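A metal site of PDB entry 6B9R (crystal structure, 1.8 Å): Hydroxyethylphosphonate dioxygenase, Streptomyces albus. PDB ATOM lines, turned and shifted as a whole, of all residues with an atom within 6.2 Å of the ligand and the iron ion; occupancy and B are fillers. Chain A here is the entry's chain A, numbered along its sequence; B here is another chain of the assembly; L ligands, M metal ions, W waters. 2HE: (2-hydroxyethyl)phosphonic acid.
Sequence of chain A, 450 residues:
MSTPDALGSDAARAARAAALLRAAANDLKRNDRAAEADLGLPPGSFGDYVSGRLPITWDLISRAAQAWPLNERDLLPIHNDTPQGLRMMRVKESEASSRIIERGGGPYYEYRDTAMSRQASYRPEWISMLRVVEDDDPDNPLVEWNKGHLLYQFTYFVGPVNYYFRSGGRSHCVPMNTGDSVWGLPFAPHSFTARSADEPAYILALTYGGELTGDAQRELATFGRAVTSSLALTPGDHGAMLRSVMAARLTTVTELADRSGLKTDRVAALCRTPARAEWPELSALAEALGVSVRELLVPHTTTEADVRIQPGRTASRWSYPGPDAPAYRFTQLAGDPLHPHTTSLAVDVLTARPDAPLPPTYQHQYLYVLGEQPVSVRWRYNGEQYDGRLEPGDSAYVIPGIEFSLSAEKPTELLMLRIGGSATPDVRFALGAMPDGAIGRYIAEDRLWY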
ATOM      1  N   ARG A 103     -37.412 -27.105  -7.544  1.00  0.00           N
ATOM      2  CA  ARG A 103     -38.121 -27.184  -6.282  1.00  0.00           C
ATOM      3  C   ARG A 103     -39.070 -26.006  -6.201  1.00  0.00           C
ATOM      4  O   ARG A 103     -38.702 -24.880  -6.540  1.00  0.00           O
ATOM      5  CB  ARG A 103     -37.165 -27.154  -5.081  1.00  0.00           C
ATOM      6  CG  ARG A 103     -36.210 -28.324  -4.960  1.00  0.00           C
ATOM      7  CD  ARG A 103     -35.392 -28.168  -3.693  1.00  0.00           C
ATOM      8  NE  ARG A 103     -34.334 -29.176  -3.550  1.00  0.00           N
ATOM      9  CZ  ARG A 103     -33.518 -29.233  -2.513  1.00  0.00           C
ATOM     10  NH1 ARG A 103     -33.629 -28.332  -1.532  1.00  0.00           N
ATOM     11  NH2 ARG A 103     -32.582 -30.178  -2.443  1.00  0.00           N
ATOM     12  N   TYR A 109     -31.414 -25.732  -7.930  1.00  0.00           N
ATOM     13  CA  TYR A 109     -29.980 -25.970  -7.888  1.00  0.00           C
ATOM     14  C   TYR A 109     -29.514 -26.529  -9.231  1.00  0.00           C
ATOM     15  O   TYR A 109     -30.271 -27.246  -9.905  1.00  0.00           O
ATOM     16  CB  TYR A 109     -29.579 -26.998  -6.828  1.00  0.00           C
ATOM     17  CG  TYR A 109     -29.835 -26.651  -5.375  1.00  0.00           C
ATOM     18  CD1 TYR A 109     -29.511 -25.400  -4.850  1.00  0.00           C
ATOM     19  CD2 TYR A 109     -30.356 -27.602  -4.510  1.00  0.00           C
ATOM     20  CE1 TYR A 109     -29.733 -25.111  -3.522  1.00  0.00           C
ATOM     21  CE2 TYR A 109     -30.570 -27.329  -3.172  1.00  0.00           C
ATOM     22  CZ  TYR A 109     -30.256 -26.079  -2.683  1.00  0.00           C
ATOM     23  OH  TYR A 109     -30.483 -25.812  -1.348  1.00  0.00           O
ATOM     24  N   TYR A 111     -26.342 -29.011 -10.007  1.00  0.00           N
ATOM     25  CA  TYR A 111     -25.294 -29.831  -9.411  1.00  0.00           C
ATOM     26  C   TYR A 111     -24.270 -30.241 -10.458  1.00  0.00           C
ATOM     27  O   TYR A 111     -24.618 -30.554 -11.604  1.00  0.00           O
ATOM     28  CB  TYR A 111     -25.861 -31.124  -8.812  1.00  0.00           C
ATOM     29  CG  TYR A 111     -26.894 -31.003  -7.715  1.00  0.00           C
ATOM     30  CD1 TYR A 111     -28.246 -30.870  -8.023  1.00  0.00           C
ATOM     31  CD2 TYR A 111     -26.531 -31.073  -6.382  1.00  0.00           C
ATOM     32  CE1 TYR A 111     -29.201 -30.801  -7.036  1.00  0.00           C
ATOM     33  CE2 TYR A 111     -27.483 -31.002  -5.371  1.00  0.00           C
ATOM     34  CZ  TYR A 111     -28.821 -30.856  -5.711  1.00  0.00           C
ATOM     35  OH  TYR A 111     -29.771 -30.795  -4.720  1.00  0.00           O
ATOM     36  N   ILE A 127     -22.398 -26.654  -6.570  1.00  0.00           N
ATOM     37  CA  ILE A 127     -23.839 -26.425  -6.644  1.00  0.00           C
ATOM     38  C   ILE A 127     -24.105 -24.930  -6.742  1.00  0.00           C
ATOM     39  O   ILE A 127     -23.749 -24.175  -5.832  1.00  0.00           O
ATOM     40  CB  ILE A 127     -24.594 -27.030  -5.451  1.00  0.00           C
ATOM     41  CG1 ILE A 127     -24.203 -28.504  -5.224  1.00  0.00           C
ATOM     42  CG2 ILE A 127     -26.097 -26.883  -5.676  1.00  0.00           C
ATOM     43  CD1 ILE A 127     -24.794 -29.112  -3.976  1.00  0.00           C
ATOM     44  N   GLU A 144     -36.700 -23.746  -0.349  1.00  0.00           N
ATOM     45  CA  GLU A 144     -37.109 -25.150  -0.447  1.00  0.00           C
ATOM     46  C   GLU A 144     -36.064 -25.971   0.278  1.00  0.00           C
ATOM     47  O   GLU A 144     -34.913 -26.053  -0.167  1.00  0.00           O
ATOM     48  CB  GLU A 144     -37.271 -25.582  -1.902  1.00  0.00           C
ATOM     49  CG  GLU A 144     -38.429 -24.901  -2.605  1.00  0.00           C
ATOM     50  CD  GLU A 144     -39.803 -25.402  -2.143  1.00  0.00           C
ATOM     51  OE1 GLU A 144     -39.875 -26.429  -1.425  1.00  0.00           O
ATOM     52  OE2 GLU A 144     -40.813 -24.773  -2.500  1.00  0.00           O
ATOM     53  N   TRP A 145     -36.462 -26.575   1.379  1.00  0.00           N
ATOM     54  CA  TRP A 145     -35.559 -27.274   2.276  1.00  0.00           C
ATOM     55  C   TRP A 145     -35.386 -28.717   1.815  1.00  0.00           C
ATOM     56  O   TRP A 145     -36.284 -29.300   1.204  1.00  0.00           O
ATOM     57  CB  TRP A 145     -36.104 -27.281   3.700  1.00  0.00           C
ATOM     58  CG  TRP A 145     -36.248 -25.925   4.288  1.00  0.00           C
ATOM     59  CD1 TRP A 145     -37.201 -24.995   4.015  1.00  0.00           C
ATOM     60  CD2 TRP A 145     -35.403 -25.351   5.288  1.00  0.00           C
ATOM     61  NE1 TRP A 145     -37.005 -23.869   4.769  1.00  0.00           N
ATOM     62  CE2 TRP A 145     -35.903 -24.062   5.558  1.00  0.00           C
ATOM     63  CE3 TRP A 145     -34.270 -25.806   5.969  1.00  0.00           C
ATOM     64  CZ2 TRP A 145     -35.311 -23.227   6.501  1.00  0.00           C
ATOM     65  CZ3 TRP A 145     -33.676 -24.968   6.896  1.00  0.00           C
ATOM     66  CH2 TRP A 145     -34.196 -23.698   7.149  1.00  0.00           C
ATOM     67  N   ASN A 146     -34.243 -29.295   2.130  1.00  0.00           N
ATOM     68  CA  ASN A 146     -34.090 -30.740   1.979  1.00  0.00           C
ATOM     69  C   ASN A 146     -34.536 -31.414   3.277  1.00  0.00           C
ATOM     70  O   ASN A 146     -34.952 -30.767   4.239  1.00  0.00           O
ATOM     71  CB  ASN A 146     -32.669 -31.107   1.558  1.00  0.00           C
ATOM     72  CG  ASN A 146     -31.612 -30.879   2.652  1.00  0.00           C
ATOM     73  OD1 ASN A 146     -31.915 -30.846   3.843  1.00  0.00           O
ATOM     74  ND2 ASN A 146     -30.366 -30.729   2.228  1.00  0.00           N
ATOM     75  N   LYS A 147     -34.444 -32.737   3.296  1.00  0.00           N
ATOM     76  CA  LYS A 147     -34.839 -33.522   4.448  1.00  0.00           C
ATOM     77  C   LYS A 147     -33.663 -33.864   5.350  1.00  0.00           C
ATOM     78  O   LYS A 147     -33.831 -34.612   6.322  1.00  0.00           O
ATOM     79  CB  LYS A 147     -35.526 -34.812   3.979  1.00  0.00           C
ATOM     80  CG  LYS A 147     -36.662 -34.549   2.995  1.00  0.00           C
ATOM     81  CD  LYS A 147     -37.323 -35.852   2.566  1.00  0.00           C
ATOM     82  CE  LYS A 147     -38.384 -35.623   1.487  1.00  0.00           C
ATOM     83  NZ  LYS A 147     -38.583 -36.861   0.672  1.00  0.00           N
ATOM     84  N   HIS A 149     -29.498 -35.359   5.178  1.00  0.00           N
ATOM     85  CA  HIS A 149     -28.926 -36.539   4.567  1.00  0.00           C
ATOM     86  C   HIS A 149     -27.843 -37.086   5.493  1.00  0.00           C
ATOM     87  O   HIS A 149     -27.288 -36.378   6.337  1.00  0.00           O
ATOM     88  CB  HIS A 149     -28.360 -36.216   3.175  1.00  0.00           C
ATOM     89  CG  HIS A 149     -27.487 -35.003   3.130  1.00  0.00           C
ATOM     90  ND1 HIS A 149     -26.296 -34.922   3.824  1.00  0.00           N
ATOM     91  CD2 HIS A 149     -27.617 -33.822   2.474  1.00  0.00           C
ATOM     92  CE1 HIS A 149     -25.745 -33.744   3.598  1.00  0.00           C
ATOM     93  NE2 HIS A 149     -26.517 -33.064   2.775  1.00  0.00           N
ATOM     94  N   GLN A 153     -21.480 -32.654   6.137  1.00  0.00           N
ATOM     95  CA  GLN A 153     -21.215 -31.690   5.073  1.00  0.00           C
ATOM     96  C   GLN A 153     -20.250 -30.612   5.515  1.00  0.00           C
ATOM     97  O   GLN A 153     -20.411 -30.028   6.591  1.00  0.00           O
ATOM     98  CB  GLN A 153     -22.494 -31.047   4.551  1.00  0.00           C
ATOM     99  CG  GLN A 153     -22.263 -30.307   3.241  1.00  0.00           C
ATOM    100  CD  GLN A 153     -23.577 -29.966   2.554  1.00  0.00           C
ATOM    101  OE1 GLN A 153     -24.435 -30.813   2.398  1.00  0.00           O
ATOM    102  NE2 GLN A 153     -23.723 -28.706   2.152  1.00  0.00           N
ATOM    103  N   THR A 155     -19.178 -27.086   3.730  1.00  0.00           N
ATOM    104  CA  THR A 155     -19.607 -26.231   2.633  1.00  0.00           C
ATOM    105  C   THR A 155     -18.743 -24.978   2.601  1.00  0.00           C
ATOM    106  O   THR A 155     -18.545 -24.337   3.636  1.00  0.00           O
ATOM    107  CB  THR A 155     -21.083 -25.852   2.777  1.00  0.00           C
ATOM    108  OG1 THR A 155     -21.874 -27.050   2.822  1.00  0.00           O
ATOM    109  CG2 THR A 155     -21.516 -25.011   1.595  1.00  0.00           C
ATOM    110  N   HIS A 190     -31.244 -28.495   5.531  1.00  0.00           N
ATOM    111  CA  HIS A 190     -30.648 -27.214   5.167  1.00  0.00           C
ATOM    112  C   HIS A 190     -31.053 -26.827   3.745  1.00  0.00           C
ATOM    113  O   HIS A 190     -31.622 -27.624   2.997  1.00  0.00           O
ATOM    114  CB  HIS A 190     -29.128 -27.243   5.326  1.00  0.00           C
ATOM    115  CG  HIS A 190     -28.446 -28.350   4.581  1.00  0.00           C
ATOM    116  ND1 HIS A 190     -28.357 -29.633   5.076  1.00  0.00           N
ATOM    117  CD2 HIS A 190     -27.803 -28.361   3.387  1.00  0.00           C
ATOM    118  CE1 HIS A 190     -27.706 -30.388   4.207  1.00  0.00           C
ATOM    119  NE2 HIS A 190     -27.359 -29.639   3.181  1.00  0.00           N
ATOM    120  N   SER A 191     -30.781 -25.557   3.408  1.00  0.00           N
ATOM    121  CA  SER A 191     -31.054 -25.033   2.069  1.00  0.00           C
ATOM    122  C   SER A 191     -30.100 -23.888   1.783  1.00  0.00           C
ATOM    123  O   SER A 191     -29.425 -23.373   2.670  1.00  0.00           O
ATOM    124  CB  SER A 191     -32.506 -24.579   1.939  1.00  0.00           C
ATOM    125  OG  SER A 191     -32.837 -24.338   0.573  1.00  0.00           O
ATOM    126  N   PHE A 192     -30.062 -23.496   0.503  1.00  0.00           N
ATOM    127  CA  PHE A 192     -29.238 -22.378   0.040  1.00  0.00           C
ATOM    128  C   PHE A 192     -29.997 -21.574  -1.007  1.00  0.00           C
ATOM    129  O   PHE A 192     -30.665 -22.149  -1.874  1.00  0.00           O
ATOM    130  CB  PHE A 192     -27.921 -22.836  -0.601  1.00  0.00           C
ATOM    131  CG  PHE A 192     -27.136 -23.776   0.237  1.00  0.00           C
ATOM    132  CD1 PHE A 192     -27.362 -25.147   0.154  1.00  0.00           C
ATOM    133  CD2 PHE A 192     -26.141 -23.312   1.080  1.00  0.00           C
ATOM    134  CE1 PHE A 192     -26.617 -26.052   0.913  1.00  0.00           C
ATOM    135  CE2 PHE A 192     -25.372 -24.217   1.840  1.00  0.00           C
ATOM    136  CZ  PHE A 192     -25.622 -25.587   1.756  1.00  0.00           C
ATOM    137  N   ILE A 203     -21.780 -22.944  -4.148  1.00  0.00           N
ATOM    138  CA  ILE A 203     -21.055 -23.571  -3.049  1.00  0.00           C
ATOM    139  C   ILE A 203     -20.266 -24.751  -3.578  1.00  0.00           C
ATOM    140  O   ILE A 203     -20.582 -25.342  -4.606  1.00  0.00           O
ATOM    141  CB  ILE A 203     -21.990 -24.030  -1.911  1.00  0.00           C
ATOM    142  CG1 ILE A 203     -22.920 -25.161  -2.383  1.00  0.00           C
ATOM    143  CG2 ILE A 203     -22.761 -22.840  -1.315  1.00  0.00           C
ATOM    144  CD1 ILE A 203     -23.916 -25.593  -1.320  1.00  0.00           C
ATOM    145  N   ALA A 205     -20.080 -28.025  -1.970  1.00  0.00           N
ATOM    146  CA  ALA A 205     -20.710 -28.854  -0.937  1.00  0.00           C
ATOM    147  C   ALA A 205     -19.957 -30.170  -0.882  1.00  0.00           C
ATOM    148  O   ALA A 205     -20.224 -31.091  -1.658  1.00  0.00           O
ATOM    149  CB  ALA A 205     -22.200 -29.070  -1.260  1.00  0.00           C
ATOM    150  N   THR A 207     -19.574 -33.170   0.843  1.00  0.00           N
ATOM    151  CA  THR A 207     -20.075 -34.139   1.812  1.00  0.00           C
ATOM    152  C   THR A 207     -19.163 -35.363   1.874  1.00  0.00           C
ATOM    153  O   THR A 207     -18.442 -35.682   0.926  1.00  0.00           O
ATOM    154  CB  THR A 207     -21.514 -34.575   1.478  1.00  0.00           C
ATOM    155  OG1 THR A 207     -21.524 -35.361   0.281  1.00  0.00           O
ATOM    156  CG2 THR A 207     -22.432 -33.366   1.289  1.00  0.00           C
ATOM    157  N   LYS B  29     -26.512 -37.250  -5.250  1.00  0.00           N
ATOM    158  CA  LYS B  29     -27.464 -36.269  -5.779  1.00  0.00           C
ATOM    159  C   LYS B  29     -28.049 -36.721  -7.119  1.00  0.00           C
ATOM    160  O   LYS B  29     -28.184 -35.921  -8.057  1.00  0.00           O
ATOM    161  CB  LYS B  29     -26.814 -34.885  -5.906  1.00  0.00           C
ATOM    162  CG  LYS B  29     -26.091 -34.427  -4.644  1.00  0.00           C
ATOM    163  CD  LYS B  29     -27.064 -34.207  -3.492  1.00  0.00           C
ATOM    164  CE  LYS B  29     -26.337 -33.772  -2.229  1.00  0.00           C
ATOM    165  NZ  LYS B  29     -27.315 -33.485  -1.129  1.00  0.00           N
ATOM    166  N   TRP B 449     -33.704 -37.384  -0.868  1.00  0.00           N
ATOM    167  CA  TRP B 449     -33.067 -36.427   0.034  1.00  0.00           C
ATOM    168  C   TRP B 449     -33.759 -35.069   0.065  1.00  0.00           C
ATOM    169  O   TRP B 449     -33.470 -34.273   0.950  1.00  0.00           O
ATOM    170  CB  TRP B 449     -31.564 -36.264  -0.297  1.00  0.00           C
ATOM    171  CG  TRP B 449     -31.218 -35.325  -1.426  1.00  0.00           C
ATOM    172  CD1 TRP B 449     -30.867 -34.009  -1.322  1.00  0.00           C
ATOM    173  CD2 TRP B 449     -31.169 -35.638  -2.826  1.00  0.00           C
ATOM    174  NE1 TRP B 449     -30.609 -33.480  -2.567  1.00  0.00           N
ATOM    175  CE2 TRP B 449     -30.786 -34.459  -3.512  1.00  0.00           C
ATOM    176  CE3 TRP B 449     -31.419 -36.800  -3.578  1.00  0.00           C
ATOM    177  CZ2 TRP B 449     -30.648 -34.408  -4.898  1.00  0.00           C
ATOM    178  CZ3 TRP B 449     -31.289 -36.737  -4.956  1.00  0.00           C
ATOM    179  CH2 TRP B 449     -30.904 -35.557  -5.601  1.00  0.00           C
ATOM    180  N   TYR B 450     -34.672 -34.808  -0.866  1.00  0.00           N
ATOM    181  CA  TYR B 450     -35.432 -33.551  -0.868  1.00  0.00           C
ATOM    182  C   TYR B 450     -36.888 -33.848  -1.226  1.00  0.00           C
ATOM    183  O   TYR B 450     -37.217 -34.960  -1.639  1.00  0.00           O
ATOM    184  CB  TYR B 450     -34.819 -32.557  -1.861  1.00  0.00           C
ATOM    185  CG  TYR B 450     -34.993 -32.971  -3.297  1.00  0.00           C
ATOM    186  CD1 TYR B 450     -34.146 -33.905  -3.880  1.00  0.00           C
ATOM    187  CD2 TYR B 450     -36.032 -32.459  -4.063  1.00  0.00           C
ATOM    188  CE1 TYR B 450     -34.319 -34.311  -5.197  1.00  0.00           C
ATOM    189  CE2 TYR B 450     -36.217 -32.844  -5.376  1.00  0.00           C
ATOM    190  CZ  TYR B 450     -35.358 -33.774  -5.941  1.00  0.00           C
ATOM    191  OH  TYR B 450     -35.535 -34.160  -7.242  1.00  0.00           O
ATOM    192  OXT TYR B 450     -37.772 -32.995  -1.133  1.00  0.00           O
HETATM  193  O3  2HE L   1     -28.195 -31.229   0.025  1.00  0.00           O
HETATM  194  P   2HE L   1     -28.931 -30.470  -1.011  1.00  0.00           P
HETATM  195  O1  2HE L   1     -30.465 -30.243  -0.568  1.00  0.00           O
HETATM  196  O2  2HE L   1     -28.889 -31.229  -2.441  1.00  0.00           O
HETATM  197  CA  2HE L   1     -28.091 -28.870  -1.138  1.00  0.00           C
HETATM  198  CB  2HE L   1     -26.593 -29.147  -0.999  1.00  0.00           C
HETATM  199  O4  2HE L   1     -26.220 -29.373   0.361  1.00  0.00           O
HETATM  200 FE    FE M   1     -26.461 -31.026   1.766  1.00  0.00          FE
HETATM  201  O   HOH W   1     -31.261 -28.066   0.213  1.00  0.00           O
HETATM  202  O   HOH W   2     -24.997 -31.762  -0.188  1.00  0.00           O
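An oxygen (O2) of the ligand sits at hydrogen-bond distance from the indole nitrogen (NE1) of Trp 449 of chain B (2.8 Å). NH2 of Arg 103 lies within salt-bridge range of O1 of the ligand (2.8 Å). ND2 of Asn 146 lies within hydrogen-bond range of O1 of the ligand (2.8 Å). An oxygen (O2) of the ligand is in salt-bridge range of the side-chain amino group of Lys 29 of chain B (3.0 Å). O2 of the ligand is in hydrogen-bond range of OH of Tyr 111 (2.5 Å).
The side-chain hydroxyl (OG1) of Thr 155 lies within hydrogen-bond range of the side-chain amide nitrogen (NE2) of Gln 153, 2.6 Å away. O of Glu 144 is in hydrogen-bond range of NH1 of Arg 103, 3.0 Å away. The backbone carbonyl oxygen (O) of Trp 449 of chain B sits at hydrogen-bond distance from the backbone NH (N) of Lys 147 (3.0 Å). The backbone NH (N) of Ile 203 is in hydrogen-bond range of the backbone carbonyl oxygen (O) of Ile 127 (2.9 Å). The side-chain amide oxygen (OD1) of Asn 146 sits at hydrogen-bond distance from the backbone NH (N) of His 190. The side-chain hydroxyl (OH) of Tyr 109 lies within hydrogen-bond range of the side-chain hydroxyl (OG) of Ser 191. The backbone NH (N) of Phe 192 is in hydrogen-bond range of the side-chain hydroxyl (OH) of Tyr 109 (3.0 Å).
Tyr 109 touches the ligand. CD1 of Ile 127 touches CB of the ligand (3.5 Å). Phe 192 touches the ligand. The nearest printed residue that does not touch the ligand is Ala 205 (4.3 Å).
Merely in contact with the iron ion: Asn 146 (3.9 Å) and Lys 29 of chain B (3.9 Å). Five residues have an atom within 4 Å of the iron ion: Asn 146, His 149, Gln 153, His 190 and Lys 29 of chain B.
The iron ion is bound by the side-chain amide oxygen (OE1) of Gln 153. NE2 of His 190 is bound to the iron ion. O4 of the ligand binds the iron ion. The iron ion is bound by NE2 of His 149. O3 of the ligand binds the iron ion, at 2.5 Å. Water W2 is bound to the iron ion (2.6 Å).
Water W1 lies within hydrogen-bond range of an oxygen (O1) of the ligand (2.4 Å), the backbone carbonyl oxygen (O) of His 190 (2.8 Å), the side-chain hydroxyl (OH) of Tyr 109 (2.9 Å), the guanidinium group (NH1) of Arg 103 (3.0 Å) and the side-chain amide nitrogen (ND2) of Asn 146 (3.5 Å).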
